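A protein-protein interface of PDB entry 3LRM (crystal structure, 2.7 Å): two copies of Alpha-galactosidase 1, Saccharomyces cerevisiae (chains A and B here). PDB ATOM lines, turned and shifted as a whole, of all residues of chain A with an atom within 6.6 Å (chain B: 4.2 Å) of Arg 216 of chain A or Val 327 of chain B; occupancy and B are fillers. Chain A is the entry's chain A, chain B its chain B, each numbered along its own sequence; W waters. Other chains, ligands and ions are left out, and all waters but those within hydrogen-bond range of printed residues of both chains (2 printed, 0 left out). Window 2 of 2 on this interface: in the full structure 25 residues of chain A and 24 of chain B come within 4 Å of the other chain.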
ATOM      1  N   THR A 211      -8.056  12.289   6.673  1.00  0.00           N
ATOM      2  CA  THR A 211      -9.438  11.870   6.542  1.00  0.00           C
ATOM      3  C   THR A 211     -10.188  12.928   5.736  1.00  0.00           C
ATOM      4  O   THR A 211      -9.693  14.045   5.564  1.00  0.00           O
ATOM      5  CB  THR A 211     -10.092  11.648   7.919  1.00  0.00           C
ATOM      6  OG1 THR A 211     -11.407  11.115   7.740  1.00  0.00           O
ATOM      7  CG2 THR A 211     -10.165  12.948   8.723  1.00  0.00           C
ATOM      8  N   GLU A 213     -12.039  15.243   6.182  1.00  0.00           N
ATOM      9  CA  GLU A 213     -12.475  16.380   6.996  1.00  0.00           C
ATOM     10  C   GLU A 213     -11.497  17.530   6.787  1.00  0.00           C
ATOM     11  O   GLU A 213     -10.283  17.336   6.795  1.00  0.00           O
ATOM     12  CB  GLU A 213     -12.525  16.013   8.483  1.00  0.00           C
ATOM     13  CG  GLU A 213     -13.533  14.923   8.853  1.00  0.00           C
ATOM     14  CD  GLU A 213     -14.977  15.396   8.826  1.00  0.00           C
ATOM     15  OE1 GLU A 213     -15.220  16.600   9.057  1.00  0.00           O
ATOM     16  OE2 GLU A 213     -15.865  14.551   8.583  1.00  0.00           O
ATOM     17  N   PHE A 214     -12.023  18.730   6.597  1.00  0.00           N
ATOM     18  CA  PHE A 214     -11.170  19.883   6.363  1.00  0.00           C
ATOM     19  C   PHE A 214     -10.543  20.442   7.644  1.00  0.00           C
ATOM     20  O   PHE A 214      -9.367  20.784   7.654  1.00  0.00           O
ATOM     21  CB  PHE A 214     -11.918  20.970   5.584  1.00  0.00           C
ATOM     22  CG  PHE A 214     -11.011  21.961   4.905  1.00  0.00           C
ATOM     23  CD1 PHE A 214     -10.200  21.573   3.840  1.00  0.00           C
ATOM     24  CD2 PHE A 214     -10.972  23.282   5.322  1.00  0.00           C
ATOM     25  CE1 PHE A 214      -9.357  22.487   3.213  1.00  0.00           C
ATOM     26  CE2 PHE A 214     -10.128  24.202   4.707  1.00  0.00           C
ATOM     27  CZ  PHE A 214      -9.321  23.805   3.651  1.00  0.00           C
ATOM     28  N   THR A 215     -11.310  20.515   8.728  1.00  0.00           N
ATOM     29  CA  THR A 215     -10.818  21.137   9.959  1.00  0.00           C
ATOM     30  C   THR A 215     -11.003  20.297  11.212  1.00  0.00           C
ATOM     31  O   THR A 215     -10.281  20.489  12.187  1.00  0.00           O
ATOM     32  CB  THR A 215     -11.494  22.498  10.237  1.00  0.00           C
ATOM     33  OG1 THR A 215     -12.874  22.288  10.549  1.00  0.00           O
ATOM     34  CG2 THR A 215     -11.366  23.456   9.051  1.00  0.00           C
ATOM     35  N   ARG A 216     -11.964  19.376  11.185  1.00  0.00           N
ATOM     36  CA  ARG A 216     -12.393  18.609  12.371  1.00  0.00           C
ATOM     37  C   ARG A 216     -11.272  18.013  13.220  1.00  0.00           C
ATOM     38  O   ARG A 216     -10.551  17.131  12.762  1.00  0.00           O
ATOM     39  CB  ARG A 216     -13.349  17.482  11.959  1.00  0.00           C
ATOM     40  CG  ARG A 216     -14.143  16.901  13.122  1.00  0.00           C
ATOM     41  CD  ARG A 216     -14.707  15.522  12.808  1.00  0.00           C
ATOM     42  NE  ARG A 216     -15.718  15.139  13.793  1.00  0.00           N
ATOM     43  CZ  ARG A 216     -15.467  14.544  14.961  1.00  0.00           C
ATOM     44  NH1 ARG A 216     -14.225  14.237  15.318  1.00  0.00           N
ATOM     45  NH2 ARG A 216     -16.468  14.255  15.779  1.00  0.00           N
ATOM     46  N   PRO A 217     -11.128  18.486  14.473  1.00  0.00           N
ATOM     47  CA  PRO A 217     -10.265  17.783  15.420  1.00  0.00           C
ATOM     48  C   PRO A 217     -10.843  16.410  15.768  1.00  0.00           C
ATOM     49  O   PRO A 217     -12.064  16.239  15.781  1.00  0.00           O
ATOM     50  CB  PRO A 217     -10.285  18.692  16.654  1.00  0.00           C
ATOM     51  CG  PRO A 217     -10.715  20.022  16.151  1.00  0.00           C
ATOM     52  CD  PRO A 217     -11.680  19.718  15.061  1.00  0.00           C
ATOM     53  N   ASP A 218      -9.970  15.446  16.039  1.00  0.00           N
ATOM     54  CA  ASP A 218     -10.390  14.070  16.289  1.00  0.00           C
ATOM     55  C   ASP A 218      -9.587  13.481  17.430  1.00  0.00           C
ATOM     56  O   ASP A 218      -8.373  13.655  17.488  1.00  0.00           O
ATOM     57  CB  ASP A 218     -10.203  13.231  15.026  1.00  0.00           C
ATOM     58  CG  ASP A 218     -10.962  11.920  15.071  1.00  0.00           C
ATOM     59  OD1 ASP A 218     -10.635  11.051  15.906  1.00  0.00           O
ATOM     60  OD2 ASP A 218     -11.883  11.751  14.248  1.00  0.00           O
ATOM     61  N   SER A 219     -10.264  12.780  18.330  1.00  0.00           N
ATOM     62  CA  SER A 219      -9.603  12.163  19.480  1.00  0.00           C
ATOM     63  C   SER A 219      -8.568  11.109  19.072  1.00  0.00           C
ATOM     64  O   SER A 219      -7.654  10.802  19.836  1.00  0.00           O
ATOM     65  CB  SER A 219     -10.632  11.565  20.433  1.00  0.00           C
ATOM     66  OG  SER A 219     -11.212  10.406  19.871  1.00  0.00           O
ATOM     67  N   ARG A 220      -8.711  10.569  17.866  1.00  0.00           N
ATOM     68  CA  ARG A 220      -7.748   9.601  17.330  1.00  0.00           C
ATOM     69  C   ARG A 220      -6.515  10.274  16.720  1.00  0.00           C
ATOM     70  O   ARG A 220      -5.566   9.599  16.341  1.00  0.00           O
ATOM     71  CB  ARG A 220      -8.416   8.699  16.293  1.00  0.00           C
ATOM     72  CG  ARG A 220      -9.434   7.728  16.866  1.00  0.00           C
ATOM     73  CD  ARG A 220     -10.361   7.175  15.802  1.00  0.00           C
ATOM     74  NE  ARG A 220     -11.139   8.234  15.162  1.00  0.00           N
ATOM     75  CZ  ARG A 220     -11.977   8.061  14.141  1.00  0.00           C
ATOM     76  NH1 ARG A 220     -12.180   6.857  13.623  1.00  0.00           N
ATOM     77  NH2 ARG A 220     -12.614   9.106  13.636  1.00  0.00           N
ATOM     78  N   HIS A 236      -7.048   9.810  11.275  1.00  0.00           N
ATOM     79  CA  HIS A 236      -8.246  10.644  11.153  1.00  0.00           C
ATOM     80  C   HIS A 236      -7.938  12.102  11.456  1.00  0.00           C
ATOM     81  O   HIS A 236      -8.750  12.820  12.040  1.00  0.00           O
ATOM     82  CB  HIS A 236      -9.398  10.123  12.011  1.00  0.00           C
ATOM     83  CG  HIS A 236      -9.977   8.844  11.507  1.00  0.00           C
ATOM     84  ND1 HIS A 236     -11.044   8.801  10.637  1.00  0.00           N
ATOM     85  CD2 HIS A 236      -9.615   7.559  11.723  1.00  0.00           C
ATOM     86  CE1 HIS A 236     -11.324   7.542  10.349  1.00  0.00           C
ATOM     87  NE2 HIS A 236     -10.474   6.768  10.999  1.00  0.00           N
ATOM     88  N   CYS A 237      -6.750  12.523  11.037  1.00  0.00           N
ATOM     89  CA  CYS A 237      -6.332  13.907  11.131  1.00  0.00           C
ATOM     90  C   CYS A 237      -6.964  14.682   9.988  1.00  0.00           C
ATOM     91  O   CYS A 237      -7.095  14.167   8.875  1.00  0.00           O
ATOM     92  CB  CYS A 237      -4.811  13.995  11.069  1.00  0.00           C
ATOM     93  SG  CYS A 237      -4.004  13.011  12.331  1.00  0.00           S
ATOM     94  N   SER A 238      -7.371  15.912  10.275  1.00  0.00           N
ATOM     95  CA  SER A 238      -8.004  16.767   9.276  1.00  0.00           C
ATOM     96  C   SER A 238      -6.983  17.324   8.293  1.00  0.00           C
ATOM     97  O   SER A 238      -5.784  17.370   8.586  1.00  0.00           O
ATOM     98  CB  SER A 238      -8.730  17.924   9.948  1.00  0.00           C
ATOM     99  OG  SER A 238      -7.795  18.862  10.444  1.00  0.00           O
ATOM    100  N   ILE A 239      -7.476  17.756   7.135  1.00  0.00           N
ATOM    101  CA  ILE A 239      -6.645  18.369   6.098  1.00  0.00           C
ATOM    102  C   ILE A 239      -5.840  19.550   6.645  1.00  0.00           C
ATOM    103  O   ILE A 239      -4.645  19.660   6.378  1.00  0.00           O
ATOM    104  CB  ILE A 239      -7.495  18.768   4.855  1.00  0.00           C
ATOM    105  CG1 ILE A 239      -7.928  17.506   4.093  1.00  0.00           C
ATOM    106  CG2 ILE A 239      -6.727  19.697   3.928  1.00  0.00           C
ATOM    107  CD1 ILE A 239      -9.219  17.651   3.299  1.00  0.00           C
ATOM    108  N   ASN A 241      -5.144  20.112   9.865  1.00  0.00           N
ATOM    109  CA  ASN A 241      -4.250  19.590  10.890  1.00  0.00           C
ATOM    110  C   ASN A 241      -2.900  19.175  10.308  1.00  0.00           C
ATOM    111  O   ASN A 241      -1.846  19.467  10.887  1.00  0.00           O
ATOM    112  CB  ASN A 241      -4.911  18.422  11.619  1.00  0.00           C
ATOM    113  CG  ASN A 241      -4.040  17.838  12.713  1.00  0.00           C
ATOM    114  OD1 ASN A 241      -3.183  16.992  12.453  1.00  0.00           O
ATOM    115  ND2 ASN A 241      -4.268  18.268  13.950  1.00  0.00           N
ATOM    116  N   ASP A 336     -16.292  27.235  12.308  1.00  0.00           N
ATOM    117  CA  ASP A 336     -17.254  26.229  11.859  1.00  0.00           C
ATOM    118  C   ASP A 336     -17.875  25.455  13.022  1.00  0.00           C
ATOM    119  O   ASP A 336     -17.674  25.803  14.195  1.00  0.00           O
ATOM    120  CB  ASP A 336     -16.616  25.269  10.840  1.00  0.00           C
ATOM    121  CG  ASP A 336     -15.363  24.570  11.371  1.00  0.00           C
ATOM    122  OD1 ASP A 336     -15.106  24.577  12.592  1.00  0.00           O
ATOM    123  OD2 ASP A 336     -14.625  24.004  10.542  1.00  0.00           O
ATOM    124  N   TYR A 338     -17.031  22.972  14.382  1.00  0.00           N
ATOM    125  CA  TYR A 338     -16.018  22.380  15.243  1.00  0.00           C
ATOM    126  C   TYR A 338     -15.143  23.423  15.948  1.00  0.00           C
ATOM    127  O   TYR A 338     -14.119  23.078  16.548  1.00  0.00           O
ATOM    128  CB  TYR A 338     -15.150  21.405  14.442  1.00  0.00           C
ATOM    129  CG  TYR A 338     -15.928  20.358  13.680  1.00  0.00           C
ATOM    130  CD1 TYR A 338     -15.805  20.238  12.296  1.00  0.00           C
ATOM    131  CD2 TYR A 338     -16.788  19.483  14.341  1.00  0.00           C
ATOM    132  CE1 TYR A 338     -16.520  19.266  11.590  1.00  0.00           C
ATOM    133  CE2 TYR A 338     -17.505  18.512  13.651  1.00  0.00           C
ATOM    134  CZ  TYR A 338     -17.369  18.409  12.278  1.00  0.00           C
ATOM    135  OH  TYR A 338     -18.088  17.449  11.600  1.00  0.00           O
ATOM    136  N   GLN A 340     -13.316  25.670  14.595  1.00  0.00           N
ATOM    137  CA  GLN A 340     -12.100  25.907  13.836  1.00  0.00           C
ATOM    138  C   GLN A 340     -12.310  27.032  12.839  1.00  0.00           C
ATOM    139  O   GLN A 340     -13.358  27.117  12.206  1.00  0.00           O
ATOM    140  CB  GLN A 340     -11.685  24.644  13.086  1.00  0.00           C
ATOM    141  CG  GLN A 340     -11.498  23.422  13.948  1.00  0.00           C
ATOM    142  CD  GLN A 340     -10.491  23.644  15.051  1.00  0.00           C
ATOM    143  OE1 GLN A 340      -9.311  23.893  14.793  1.00  0.00           O
ATOM    144  NE2 GLN A 340     -10.952  23.551  16.298  1.00  0.00           N
ATOM    145  N   THR B 325     -14.654   4.786  20.053  1.00  0.00           N
ATOM    146  CA  THR B 325     -14.012   6.048  19.733  1.00  0.00           C
ATOM    147  C   THR B 325     -14.787   7.166  20.404  1.00  0.00           C
ATOM    148  O   THR B 325     -16.019   7.158  20.403  1.00  0.00           O
ATOM    149  CB  THR B 325     -13.985   6.262  18.198  1.00  0.00           C
ATOM    150  OG1 THR B 325     -13.093   5.311  17.605  1.00  0.00           O
ATOM    151  CG2 THR B 325     -13.528   7.663  17.831  1.00  0.00           C
ATOM    152  N   ARG B 326     -14.072   8.114  20.999  1.00  0.00           N
ATOM    153  CA  ARG B 326     -14.713   9.316  21.523  1.00  0.00           C
ATOM    154  C   ARG B 326     -15.001  10.256  20.356  1.00  0.00           C
ATOM    155  O   ARG B 326     -14.083  10.731  19.687  1.00  0.00           O
ATOM    156  CB  ARG B 326     -13.836  10.002  22.564  1.00  0.00           C
ATOM    157  CG  ARG B 326     -14.581  10.992  23.422  1.00  0.00           C
ATOM    158  CD  ARG B 326     -13.744  12.219  23.662  1.00  0.00           C
ATOM    159  NE  ARG B 326     -12.784  12.074  24.751  1.00  0.00           N
ATOM    160  CZ  ARG B 326     -11.598  12.676  24.789  1.00  0.00           C
ATOM    161  NH1 ARG B 326     -11.201  13.445  23.782  1.00  0.00           N
ATOM    162  NH2 ARG B 326     -10.799  12.499  25.833  1.00  0.00           N
ATOM    163  N   VAL B 327     -16.282  10.509  20.106  1.00  0.00           N
ATOM    164  CA  VAL B 327     -16.694  11.314  18.959  1.00  0.00           C
ATOM    165  C   VAL B 327     -16.578  12.809  19.248  1.00  0.00           C
ATOM    166  O   VAL B 327     -16.082  13.571  18.417  1.00  0.00           O
ATOM    167  CB  VAL B 327     -18.123  10.944  18.482  1.00  0.00           C
ATOM    168  CG1 VAL B 327     -18.586  11.874  17.364  1.00  0.00           C
ATOM    169  CG2 VAL B 327     -18.148   9.505  18.008  1.00  0.00           C
ATOM    170  N   TRP B 328     -17.047  13.227  20.417  1.00  0.00           N
ATOM    171  CA  TRP B 328     -16.863  14.611  20.845  1.00  0.00           C
ATOM    172  C   TRP B 328     -16.714  14.781  22.350  1.00  0.00           C
ATOM    173  O   TRP B 328     -17.033  13.885  23.127  1.00  0.00           O
ATOM    174  CB  TRP B 328     -17.949  15.537  20.282  1.00  0.00           C
ATOM    175  CG  TRP B 328     -19.390  15.109  20.488  1.00  0.00           C
ATOM    176  CD1 TRP B 328     -20.241  14.616  19.533  1.00  0.00           C
ATOM    177  CD2 TRP B 328     -20.156  15.186  21.699  1.00  0.00           C
ATOM    178  NE1 TRP B 328     -21.477  14.365  20.078  1.00  0.00           N
ATOM    179  CE2 TRP B 328     -21.454  14.713  21.402  1.00  0.00           C
ATOM    180  CE3 TRP B 328     -19.871  15.607  23.004  1.00  0.00           C
ATOM    181  CZ2 TRP B 328     -22.465  14.642  22.369  1.00  0.00           C
ATOM    182  CZ3 TRP B 328     -20.872  15.534  23.963  1.00  0.00           C
ATOM    183  CH2 TRP B 328     -22.156  15.054  23.638  1.00  0.00           C
ATOM    184  N   MET B 345     -19.354  12.022  24.074  1.00  0.00           N
ATOM    185  CA  MET B 345     -20.050  11.002  23.306  1.00  0.00           C
ATOM    186  C   MET B 345     -19.051  10.006  22.740  1.00  0.00           C
ATOM    187  O   MET B 345     -18.031  10.393  22.174  1.00  0.00           O
ATOM    188  CB  MET B 345     -20.835  11.617  22.158  1.00  0.00           C
ATOM    189  CG  MET B 345     -21.995  10.756  21.695  1.00  0.00           C
ATOM    190  SD  MET B 345     -22.014  10.492  19.926  1.00  0.00           S
ATOM    191  CE  MET B 345     -21.187   8.927  19.840  1.00  0.00           C
ATOM    192  N   SER B 347     -18.755   6.298  20.367  1.00  0.00           N
ATOM    193  CA  SER B 347     -19.409   5.359  19.483  1.00  0.00           C
ATOM    194  C   SER B 347     -18.416   4.280  19.092  1.00  0.00           C
ATOM    195  O   SER B 347     -17.212   4.536  19.010  1.00  0.00           O
ATOM    196  CB  SER B 347     -19.940   6.079  18.243  1.00  0.00           C
ATOM    197  OG  SER B 347     -20.692   5.213  17.410  1.00  0.00           O
ATOM    198  N   GLU B 375     -23.420  11.622  13.669  1.00  0.00           N
ATOM    199  CA  GLU B 375     -22.447  11.634  14.756  1.00  0.00           C
ATOM    200  C   GLU B 375     -22.120  10.224  15.232  1.00  0.00           C
ATOM    201  O   GLU B 375     -20.970   9.934  15.570  1.00  0.00           O
ATOM    202  CB  GLU B 375     -22.938  12.480  15.934  1.00  0.00           C
ATOM    203  CG  GLU B 375     -22.970  13.980  15.666  1.00  0.00           C
ATOM    204  CD  GLU B 375     -23.313  14.807  16.896  1.00  0.00           C
ATOM    205  OE1 GLU B 375     -23.955  14.281  17.836  1.00  0.00           O
ATOM    206  OE2 GLU B 375     -22.941  16.000  16.913  1.00  0.00           O
ATOM    207  N   PHE B 378     -19.596   7.945  12.650  1.00  0.00           N
ATOM    208  CA  PHE B 378     -18.655   9.044  12.429  1.00  0.00           C
ATOM    209  C   PHE B 378     -17.766   8.882  11.194  1.00  0.00           C
ATOM    210  O   PHE B 378     -17.301   9.876  10.629  1.00  0.00           O
ATOM    211  CB  PHE B 378     -17.790   9.251  13.681  1.00  0.00           C
ATOM    212  CG  PHE B 378     -17.218   7.973  14.253  1.00  0.00           C
ATOM    213  CD1 PHE B 378     -16.006   7.468  13.792  1.00  0.00           C
ATOM    214  CD2 PHE B 378     -17.887   7.278  15.260  1.00  0.00           C
ATOM    215  CE1 PHE B 378     -15.475   6.287  14.314  1.00  0.00           C
ATOM    216  CE2 PHE B 378     -17.361   6.098  15.789  1.00  0.00           C
ATOM    217  CZ  PHE B 378     -16.156   5.604  15.315  1.00  0.00           C
HETATM  218  O   HOH W   1     -13.203  13.296  18.005  1.00  0.00           O
HETATM  219  O   HOH W   2     -11.270   7.805  20.438  1.00  0.00           O
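The backbone carbonyl oxygen of Val 327 of chain B lies within hydrogen-bond range of the guanidinium group of Arg 216 of chain A.
The backbone carbonyl oxygen of Arg 326 of chain B is in hydrogen-bond range of the side-chain hydroxyl of Ser 219 of chain A (2.9 Å).
The side-chain carboxylate of Asp 218 of chain A is in salt-bridge range of the guanidinium group of Arg 216 of chain A (3.6 Å).
The guanidinium group of Arg 220 of chain A is in salt-bridge range of the side-chain carboxylate of Asp 218 of chain A (2.8 Å).
A ring nitrogen (NE2) of His 236 of chain A sits at hydrogen-bond distance from the guanidinium group (NH1) of Arg 220 of chain A, at 3.1 Å.
N of Thr 325 of chain B sits at hydrogen-bond distance from O of Ser 347 of chain B.
The backbone carbonyl oxygen (O) of Met 345 of chain B is in hydrogen-bond range of the backbone NH (N) of Val 327 of chain B.
Among the printed residues, pairs that only touch across the chains: Arg 220 of chain A with Thr 325 of chain B (3.6 Å) and Arg 220 of chain A with Phe 378 of chain B (3.4 Å).
Arg 216 of chain A touches one residue of chain B.
Of the printed residues of chain B, Ser 219 of chain A touches Arg 326 (2.9 Å).
Of the printed residues of chain A, Arg 326 of chain B touches Ser 219 (2.9 Å).
Val 327 of chain B touches just one residue of chain A: Arg 216.
The nearest residue of chain A that does not touch Val 327 of chain B is Ser 219 of chain A (5.1 Å).
The nearest printed residue of chain B that does not touch Ser 219 of chain A is Thr 325 of chain B (4.1 Å).
Hydrophobic or aromatic side chains of chain B that line the printed part of chain A: Val 327 and Phe 378.
Of the 17 printed residues of chain A, 3 touch a printed residue of chain B.
Among the printed residues, 4 pairs touch across the chains.
Among the printed residues, no Asp or Glu carboxylate lies within 4 Å of a Lys or Arg side-chain nitrogen of the other chain.
No position is printed for both chains.
Of the 4 pairs that touch across the chains among the printed residues, none has its exchanged pair printed and touching as well.
Water W2 bridges the side-chain hydroxyl (OG) of Ser 219 of chain A (2.7 Å) and the backbone NH (N) of Arg 326 of chain B (2.9 Å).
Water W1 lies within hydrogen-bond range of O of Val 327 of chain B (2.9 Å), N of Ser 219 of chain A (3.0 Å), NH1 of Arg 216 of chain A (3.0 Å) and O of Arg 326 of chain B (3.2 Å).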
